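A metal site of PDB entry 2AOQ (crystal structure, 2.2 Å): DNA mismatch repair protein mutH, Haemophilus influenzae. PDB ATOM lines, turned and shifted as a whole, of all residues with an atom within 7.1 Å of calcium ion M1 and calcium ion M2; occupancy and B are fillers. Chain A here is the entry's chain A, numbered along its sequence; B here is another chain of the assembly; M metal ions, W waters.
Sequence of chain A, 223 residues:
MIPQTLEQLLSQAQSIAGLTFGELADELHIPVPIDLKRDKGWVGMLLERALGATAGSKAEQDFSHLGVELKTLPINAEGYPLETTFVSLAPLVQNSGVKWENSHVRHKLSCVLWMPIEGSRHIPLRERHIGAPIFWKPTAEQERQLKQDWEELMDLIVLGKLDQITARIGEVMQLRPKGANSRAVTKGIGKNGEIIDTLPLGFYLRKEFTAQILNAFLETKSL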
ATOM      1  N   GLY A  44     -22.774 -26.610  -7.246  1.00  0.00           N
ATOM      2  CA  GLY A  44     -21.536 -27.100  -7.816  1.00  0.00           C
ATOM      3  C   GLY A  44     -20.538 -25.975  -7.904  1.00  0.00           C
ATOM      4  O   GLY A  44     -19.394 -26.102  -7.496  1.00  0.00           O
ATOM      5  N   MET A  45     -20.976 -24.831  -8.417  1.00  0.00           N
ATOM      6  CA  MET A  45     -20.082 -23.703  -8.564  1.00  0.00           C
ATOM      7  C   MET A  45     -19.628 -23.136  -7.230  1.00  0.00           C
ATOM      8  O   MET A  45     -18.487 -22.668  -7.077  1.00  0.00           O
ATOM      9  CB  MET A  45     -20.747 -22.608  -9.387  1.00  0.00           C
ATOM     10  CG  MET A  45     -21.033 -23.021 -10.857  1.00  0.00           C
ATOM     11  SD  MET A  45     -19.557 -23.771 -11.702  1.00  0.00           S
ATOM     12  CE  MET A  45     -19.843 -23.443 -13.542  1.00  0.00           C
ATOM     13  N   GLU A  48     -16.775 -25.137  -6.191  1.00  0.00           N
ATOM     14  CA  GLU A  48     -15.571 -24.911  -6.982  1.00  0.00           C
ATOM     15  C   GLU A  48     -14.804 -23.698  -6.461  1.00  0.00           C
ATOM     16  O   GLU A  48     -13.586 -23.731  -6.271  1.00  0.00           O
ATOM     17  CB  GLU A  48     -15.918 -24.722  -8.454  1.00  0.00           C
ATOM     18  CG  GLU A  48     -16.431 -25.969  -9.129  1.00  0.00           C
ATOM     19  CD  GLU A  48     -16.378 -25.861 -10.641  1.00  0.00           C
ATOM     20  OE1 GLU A  48     -16.832 -24.827 -11.169  1.00  0.00           O
ATOM     21  OE2 GLU A  48     -15.901 -26.811 -11.291  1.00  0.00           O
ATOM     22  N   ALA A  53     -11.081 -24.686  -7.357  1.00  0.00           N
ATOM     23  CA  ALA A  53     -11.110 -25.538  -8.539  1.00  0.00           C
ATOM     24  C   ALA A  53     -11.248 -24.704  -9.814  1.00  0.00           C
ATOM     25  O   ALA A  53     -11.588 -23.518  -9.762  1.00  0.00           O
ATOM     26  CB  ALA A  53     -12.267 -26.520  -8.450  1.00  0.00           C
ATOM     27  N   THR A  54     -10.976 -25.334 -10.957  1.00  0.00           N
ATOM     28  CA  THR A  54     -11.087 -24.661 -12.252  1.00  0.00           C
ATOM     29  C   THR A  54     -12.559 -24.377 -12.540  1.00  0.00           C
ATOM     30  O   THR A  54     -13.392 -25.293 -12.520  1.00  0.00           O
ATOM     31  CB  THR A  54     -10.531 -25.530 -13.400  1.00  0.00           C
ATOM     32  OG1 THR A  54      -9.231 -26.025 -13.069  1.00  0.00           O
ATOM     33  CG2 THR A  54     -10.420 -24.713 -14.680  1.00  0.00           C
ATOM     34  N   ALA A  55     -12.877 -23.109 -12.793  1.00  0.00           N
ATOM     35  CA  ALA A  55     -14.241 -22.701 -13.109  1.00  0.00           C
ATOM     36  C   ALA A  55     -14.441 -22.763 -14.612  1.00  0.00           C
ATOM     37  O   ALA A  55     -13.624 -23.333 -15.335  1.00  0.00           O
ATOM     38  CB  ALA A  55     -14.495 -21.285 -12.596  1.00  0.00           C
ATOM     39  N   GLY A  56     -15.540 -22.176 -15.073  1.00  0.00           N
ATOM     40  CA  GLY A  56     -15.816 -22.149 -16.497  1.00  0.00           C
ATOM     41  C   GLY A  56     -15.929 -23.506 -17.165  1.00  0.00           C
ATOM     42  O   GLY A  56     -16.115 -24.538 -16.503  1.00  0.00           O
ATOM     43  N   SER A  57     -15.801 -23.509 -18.488  1.00  0.00           N
ATOM     44  CA  SER A  57     -15.901 -24.741 -19.264  1.00  0.00           C
ATOM     45  C   SER A  57     -14.554 -25.408 -19.509  1.00  0.00           C
ATOM     46  O   SER A  57     -14.398 -26.183 -20.460  1.00  0.00           O
ATOM     47  CB  SER A  57     -16.599 -24.435 -20.592  1.00  0.00           C
ATOM     48  OG  SER A  57     -17.838 -23.768 -20.381  1.00  0.00           O
ATOM     49  N   LYS A  58     -13.573 -25.105 -18.656  1.00  0.00           N
ATOM     50  CA  LYS A  58     -12.250 -25.715 -18.793  1.00  0.00           C
ATOM     51  C   LYS A  58     -12.457 -27.219 -18.838  1.00  0.00           C
ATOM     52  O   LYS A  58     -13.021 -27.808 -17.910  1.00  0.00           O
ATOM     53  CB  LYS A  58     -11.366 -25.327 -17.610  1.00  0.00           C
ATOM     54  N   GLU A  60     -12.673 -31.144 -18.740  1.00  0.00           N
ATOM     55  CA  GLU A  60     -12.580 -32.283 -17.826  1.00  0.00           C
ATOM     56  C   GLU A  60     -11.861 -32.310 -16.478  1.00  0.00           C
ATOM     57  O   GLU A  60     -11.911 -33.346 -15.815  1.00  0.00           O
ATOM     58  CB  GLU A  60     -12.136 -33.512 -18.626  1.00  0.00           C
ATOM     59  N   GLN A  61     -11.176 -31.250 -16.045  1.00  0.00           N
ATOM     60  CA  GLN A  61     -10.551 -31.403 -14.731  1.00  0.00           C
ATOM     61  C   GLN A  61     -10.325 -30.203 -13.807  1.00  0.00           C
ATOM     62  O   GLN A  61      -9.550 -29.288 -14.090  1.00  0.00           O
ATOM     63  CB  GLN A  61      -9.276 -32.250 -14.845  1.00  0.00           C
ATOM     64  CG  GLN A  61      -9.520 -33.661 -14.281  1.00  0.00           C
ATOM     65  CD  GLN A  61      -8.350 -34.608 -14.406  1.00  0.00           C
ATOM     66  OE1 GLN A  61      -7.185 -34.201 -14.390  1.00  0.00           O
ATOM     67  NE2 GLN A  61      -8.656 -35.904 -14.505  1.00  0.00           N
ATOM     68  N   ASP A  62     -11.023 -30.276 -12.685  1.00  0.00           N
ATOM     69  CA  ASP A  62     -10.999 -29.268 -11.632  1.00  0.00           C
ATOM     70  C   ASP A  62      -9.618 -29.042 -11.031  1.00  0.00           C
ATOM     71  O   ASP A  62      -9.225 -27.906 -10.770  1.00  0.00           O
ATOM     72  CB  ASP A  62     -11.997 -29.669 -10.529  1.00  0.00           C
ATOM     73  CG  ASP A  62     -13.397 -29.925 -11.073  1.00  0.00           C
ATOM     74  OD1 ASP A  62     -13.950 -29.017 -11.740  1.00  0.00           O
ATOM     75  OD2 ASP A  62     -13.939 -31.020 -10.833  1.00  0.00           O
ATOM     76  N   PHE A  63      -8.868 -30.120 -10.796  1.00  0.00           N
ATOM     77  CA  PHE A  63      -7.531 -29.989 -10.236  1.00  0.00           C
ATOM     78  C   PHE A  63      -6.570 -30.815 -11.086  1.00  0.00           C
ATOM     79  O   PHE A  63      -6.075 -31.868 -10.662  1.00  0.00           O
ATOM     80  CB  PHE A  63      -7.521 -30.471  -8.778  1.00  0.00           C
ATOM     81  CG  PHE A  63      -8.558 -29.822  -7.915  1.00  0.00           C
ATOM     82  CD1 PHE A  63      -9.758 -30.477  -7.627  1.00  0.00           C
ATOM     83  CD2 PHE A  63      -8.345 -28.553  -7.379  1.00  0.00           C
ATOM     84  CE1 PHE A  63     -10.729 -29.879  -6.824  1.00  0.00           C
ATOM     85  CE2 PHE A  63      -9.304 -27.939  -6.571  1.00  0.00           C
ATOM     86  CZ  PHE A  63     -10.503 -28.605  -6.291  1.00  0.00           C
ATOM     87  N   VAL A  68      -7.577 -34.564  -9.787  1.00  0.00           N
ATOM     88  CA  VAL A  68      -8.799 -34.798  -9.046  1.00  0.00           C
ATOM     89  C   VAL A  68      -9.978 -34.092  -9.675  1.00  0.00           C
ATOM     90  O   VAL A  68      -9.854 -32.957 -10.136  1.00  0.00           O
ATOM     91  CB  VAL A  68      -8.658 -34.347  -7.588  1.00  0.00           C
ATOM     92  CG1 VAL A  68      -9.985 -34.522  -6.854  1.00  0.00           C
ATOM     93  CG2 VAL A  68      -7.572 -35.149  -6.893  1.00  0.00           C
ATOM     94  N   GLU A  69     -11.119 -34.786  -9.703  1.00  0.00           N
ATOM     95  CA  GLU A  69     -12.382 -34.268 -10.228  1.00  0.00           C
ATOM     96  C   GLU A  69     -13.306 -34.023  -9.039  1.00  0.00           C
ATOM     97  O   GLU A  69     -13.489 -34.900  -8.204  1.00  0.00           O
ATOM     98  CB  GLU A  69     -13.048 -35.280 -11.163  1.00  0.00           C
ATOM     99  CG  GLU A  69     -14.470 -34.923 -11.589  1.00  0.00           C
ATOM    100  CD  GLU A  69     -14.552 -33.694 -12.499  1.00  0.00           C
ATOM    101  OE1 GLU A  69     -15.659 -33.129 -12.636  1.00  0.00           O
ATOM    102  OE2 GLU A  69     -13.509 -33.297 -13.093  1.00  0.00           O
ATOM    103  N   LEU A  70     -13.878 -32.828  -8.958  1.00  0.00           N
ATOM    104  CA  LEU A  70     -14.780 -32.493  -7.866  1.00  0.00           C
ATOM    105  C   LEU A  70     -16.237 -32.676  -8.286  1.00  0.00           C
ATOM    106  O   LEU A  70     -16.643 -32.303  -9.382  1.00  0.00           O
ATOM    107  CB  LEU A  70     -14.554 -31.030  -7.457  1.00  0.00           C
ATOM    108  CG  LEU A  70     -15.510 -30.426  -6.429  1.00  0.00           C
ATOM    109  CD1 LEU A  70     -15.259 -31.051  -5.072  1.00  0.00           C
ATOM    110  CD2 LEU A  70     -15.300 -28.916  -6.368  1.00  0.00           C
ATOM    111  N   LYS A  71     -17.032 -33.292  -7.408  1.00  0.00           N
ATOM    112  CA  LYS A  71     -18.449 -33.495  -7.690  1.00  0.00           C
ATOM    113  C   LYS A  71     -19.314 -33.405  -6.454  1.00  0.00           C
ATOM    114  O   LYS A  71     -19.023 -34.030  -5.455  1.00  0.00           O
ATOM    115  CB  LYS A  71     -18.683 -34.861  -8.350  1.00  0.00           C
ATOM    116  CG  LYS A  71     -18.250 -34.906  -9.794  1.00  0.00           C
ATOM    117  CD  LYS A  71     -18.750 -36.172 -10.475  1.00  0.00           C
ATOM    118  CE  LYS A  71     -18.502 -36.079 -11.961  1.00  0.00           C
ATOM    119  NZ  LYS A  71     -19.070 -34.811 -12.476  1.00  0.00           N
ATOM    120  N   THR A  72     -20.375 -32.593  -6.525  1.00  0.00           N
ATOM    121  CA  THR A  72     -21.302 -32.473  -5.408  1.00  0.00           C
ATOM    122  C   THR A  72     -22.262 -33.654  -5.542  1.00  0.00           C
ATOM    123  O   THR A  72     -22.439 -34.172  -6.637  1.00  0.00           O
ATOM    124  CB  THR A  72     -22.129 -31.183  -5.480  1.00  0.00           C
ATOM    125  OG1 THR A  72     -22.697 -31.071  -6.787  1.00  0.00           O
ATOM    126  CG2 THR A  72     -21.266 -29.967  -5.172  1.00  0.00           C
ATOM    127  P    DT B   4     -16.692 -30.966 -19.653  1.00  0.00           P
ATOM    128  OP1  DT B   4     -15.399 -31.595 -19.316  1.00  0.00           O
ATOM    129  OP2  DT B   4     -17.892 -31.823 -19.868  1.00  0.00           O
ATOM    130  O5'  DT B   4     -17.077 -29.900 -18.544  1.00  0.00           O
ATOM    131  C5'  DT B   4     -16.245 -28.763 -18.315  1.00  0.00           C
ATOM    132  C4'  DT B   4     -17.008 -27.706 -17.551  1.00  0.00           C
ATOM    133  O4'  DT B   4     -17.998 -27.089 -18.416  1.00  0.00           O
ATOM    134  C3'  DT B   4     -17.827 -28.188 -16.377  1.00  0.00           C
ATOM    135  O3'  DT B   4     -17.025 -28.423 -15.219  1.00  0.00           O
ATOM    136  C2'  DT B   4     -18.788 -27.020 -16.175  1.00  0.00           C
ATOM    137  C1'  DT B   4     -19.063 -26.589 -17.614  1.00  0.00           C
ATOM    138  N1   DT B   4     -20.336 -27.127 -18.131  1.00  0.00           N
ATOM    139  C2   DT B   4     -21.452 -26.363 -17.935  1.00  0.00           C
ATOM    140  O2   DT B   4     -21.420 -25.282 -17.361  1.00  0.00           O
ATOM    141  N3   DT B   4     -22.613 -26.898 -18.419  1.00  0.00           N
ATOM    142  C4   DT B   4     -22.775 -28.102 -19.073  1.00  0.00           C
ATOM    143  O4   DT B   4     -23.895 -28.443 -19.472  1.00  0.00           O
ATOM    144  C5   DT B   4     -21.541 -28.867 -19.242  1.00  0.00           C
ATOM    145  C7   DT B   4     -21.614 -30.203 -19.904  1.00  0.00           C
ATOM    146  C6   DT B   4     -20.405 -28.345 -18.780  1.00  0.00           C
ATOM    147  P    DG B   5     -17.435 -29.604 -14.200  1.00  0.00           P
ATOM    148  OP1  DG B   5     -16.469 -29.588 -13.082  1.00  0.00           O
ATOM    149  OP2  DG B   5     -17.646 -30.859 -14.983  1.00  0.00           O
ATOM    150  O5'  DG B   5     -18.836 -29.133 -13.618  1.00  0.00           O
ATOM    151  C5'  DG B   5     -18.925 -27.946 -12.848  1.00  0.00           C
ATOM    152  C4'  DG B   5     -20.366 -27.652 -12.488  1.00  0.00           C
ATOM    153  O4'  DG B   5     -21.121 -27.190 -13.634  1.00  0.00           O
ATOM    154  C3'  DG B   5     -21.220 -28.788 -11.966  1.00  0.00           C
ATOM    155  O3'  DG B   5     -20.851 -29.065 -10.620  1.00  0.00           O
ATOM    156  C2'  DG B   5     -22.615 -28.181 -12.058  1.00  0.00           C
ATOM    157  C1'  DG B   5     -22.501 -27.320 -13.323  1.00  0.00           C
ATOM    158  N9   DG B   5     -23.188 -27.937 -14.439  1.00  0.00           N
ATOM    159  C8   DG B   5     -22.817 -29.058 -15.149  1.00  0.00           C
ATOM    160  N7   DG B   5     -23.725 -29.432 -16.012  1.00  0.00           N
ATOM    161  C5   DG B   5     -24.731 -28.497 -15.881  1.00  0.00           C
ATOM    162  C6   DG B   5     -25.972 -28.387 -16.541  1.00  0.00           C
ATOM    163  O6   DG B   5     -26.474 -29.153 -17.384  1.00  0.00           O
ATOM    164  N1   DG B   5     -26.683 -27.264 -16.136  1.00  0.00           N
ATOM    165  C2   DG B   5     -26.245 -26.363 -15.191  1.00  0.00           C
ATOM    166  N2   DG B   5     -27.061 -25.312 -14.924  1.00  0.00           N
ATOM    167  N3   DG B   5     -25.096 -26.470 -14.543  1.00  0.00           N
ATOM    168  C4   DG B   5     -24.403 -27.544 -14.945  1.00  0.00           C
ATOM    169  P    DA B   6     -21.393 -30.379  -9.887  1.00  0.00           P
ATOM    170  OP1  DA B   6     -20.868 -30.340  -8.491  1.00  0.00           O
ATOM    171  OP2  DA B   6     -21.133 -31.556 -10.735  1.00  0.00           O
ATOM    172  O5'  DA B   6     -22.967 -30.106  -9.804  1.00  0.00           O
ATOM    173  C5'  DA B   6     -23.921 -31.072 -10.194  1.00  0.00           C
ATOM    174  C4'  DA B   6     -25.193 -30.363 -10.594  1.00  0.00           C
ATOM    175  O4'  DA B   6     -25.252 -30.217 -12.030  1.00  0.00           O
ATOM    176  C3'  DA B   6     -26.500 -31.033 -10.230  1.00  0.00           C
ATOM    177  O3'  DA B   6     -26.806 -30.691  -8.892  1.00  0.00           O
ATOM    178  C2'  DA B   6     -27.473 -30.347 -11.190  1.00  0.00           C
ATOM    179  C1'  DA B   6     -26.597 -30.086 -12.417  1.00  0.00           C
ATOM    180  N9   DA B   6     -26.844 -30.969 -13.551  1.00  0.00           N
ATOM    181  C8   DA B   6     -26.199 -32.115 -13.975  1.00  0.00           C
ATOM    182  N7   DA B   6     -26.723 -32.642 -15.055  1.00  0.00           N
ATOM    183  C5   DA B   6     -27.782 -31.792 -15.369  1.00  0.00           C
ATOM    184  C6   DA B   6     -28.727 -31.800 -16.400  1.00  0.00           C
ATOM    185  N6   DA B   6     -28.784 -32.718 -17.357  1.00  0.00           N
ATOM    186  N1   DA B   6     -29.640 -30.807 -16.414  1.00  0.00           N
ATOM    187  C2   DA B   6     -29.590 -29.874 -15.456  1.00  0.00           C
ATOM    188  N3   DA B   6     -28.753 -29.762 -14.440  1.00  0.00           N
ATOM    189  C4   DA B   6     -27.858 -30.772 -14.454  1.00  0.00           C
HETATM  190 CA    CA M   1     -14.936 -27.611 -13.253  1.00  0.00          CA
HETATM  191 CA    CA M   2     -16.229 -31.106 -11.360  1.00  0.00          CA
HETATM  192  O   HOH W   1     -16.304 -25.737 -13.821  1.00  0.00           O
HETATM  193  O   HOH W   2     -13.665 -28.768 -14.777  1.00  0.00           O
HETATM  194  O   HOH W   3     -17.013 -29.279 -10.033  1.00  0.00           O
HETATM  195  O   HOH W   4     -18.503 -31.933 -11.984  1.00  0.00           O
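Of the 21 residues printed, 4 come within 4 Å of calcium ion M2. The nearest printed residue that does not touch calcium ion M2 is Glu 48 (4.3 Å).
Water W2 lies within hydrogen-bond range of O of Lys 58 (3.3 Å) and O3' of DT 4 of chain B (3.4 Å). Water W4 lies within hydrogen-bond range of OP2 of DA 6 of chain B (2.9 Å), NZ of Lys 71 (3.0 Å) and O5' of DG 5 of chain B (3.3 Å).
Calcium ion M2 is bound by OP1 of DG 5 of chain B (2.3 Å), the backbone carbonyl oxygen (O) of Leu 70 (2.3 Å), the side-chain carboxylate (OD2) of Asp 62 (2.4 Å), water W3 (2.4 Å), the side-chain carboxylate (OE1) of Glu 69 (2.5 Å) and water W4 (2.5 Å). Slightly farther from calcium ion M2 lies OD1 of Asp 62 (3.1 Å).
Calcium ion M1 is bound by the side-chain carboxylate of Asp 62 (2.3 Å), water W2 (2.3 Å), the side-chain carboxylate of Glu 48 (2.3 Å), water W1 (2.4 Å), OP1 of DG 5 of chain B (2.5 Å) and the backbone carbonyl oxygen of Thr 54 (2.9 Å). Calcium ion M1 has six donor atoms within binding distance. Slightly farther from calcium ion M1 lies O3' of DT 4 of chain B (3.0 Å).
N of Ala 53 sits at hydrogen-bond distance from O of Glu 48, 2.9 Å away. The side-chain carboxylate (OE1) of Glu 69 lies close to the side-chain amino group (NZ) of Lys 71. O of Gln 61 lies within hydrogen-bond range of OG1 of Thr 54 (3.4 Å). N of Glu 60 lies within hydrogen-bond range of OP1 of DT 4 of chain B (2.8 Å).
Within 4 Å of calcium ion M1: Glu 48, Thr 54, Asp 62, DT 4 of chain B and DG 5 of chain B. Along chain A the residues within 4 Å of calcium ion M1 span positions 48 to 62.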
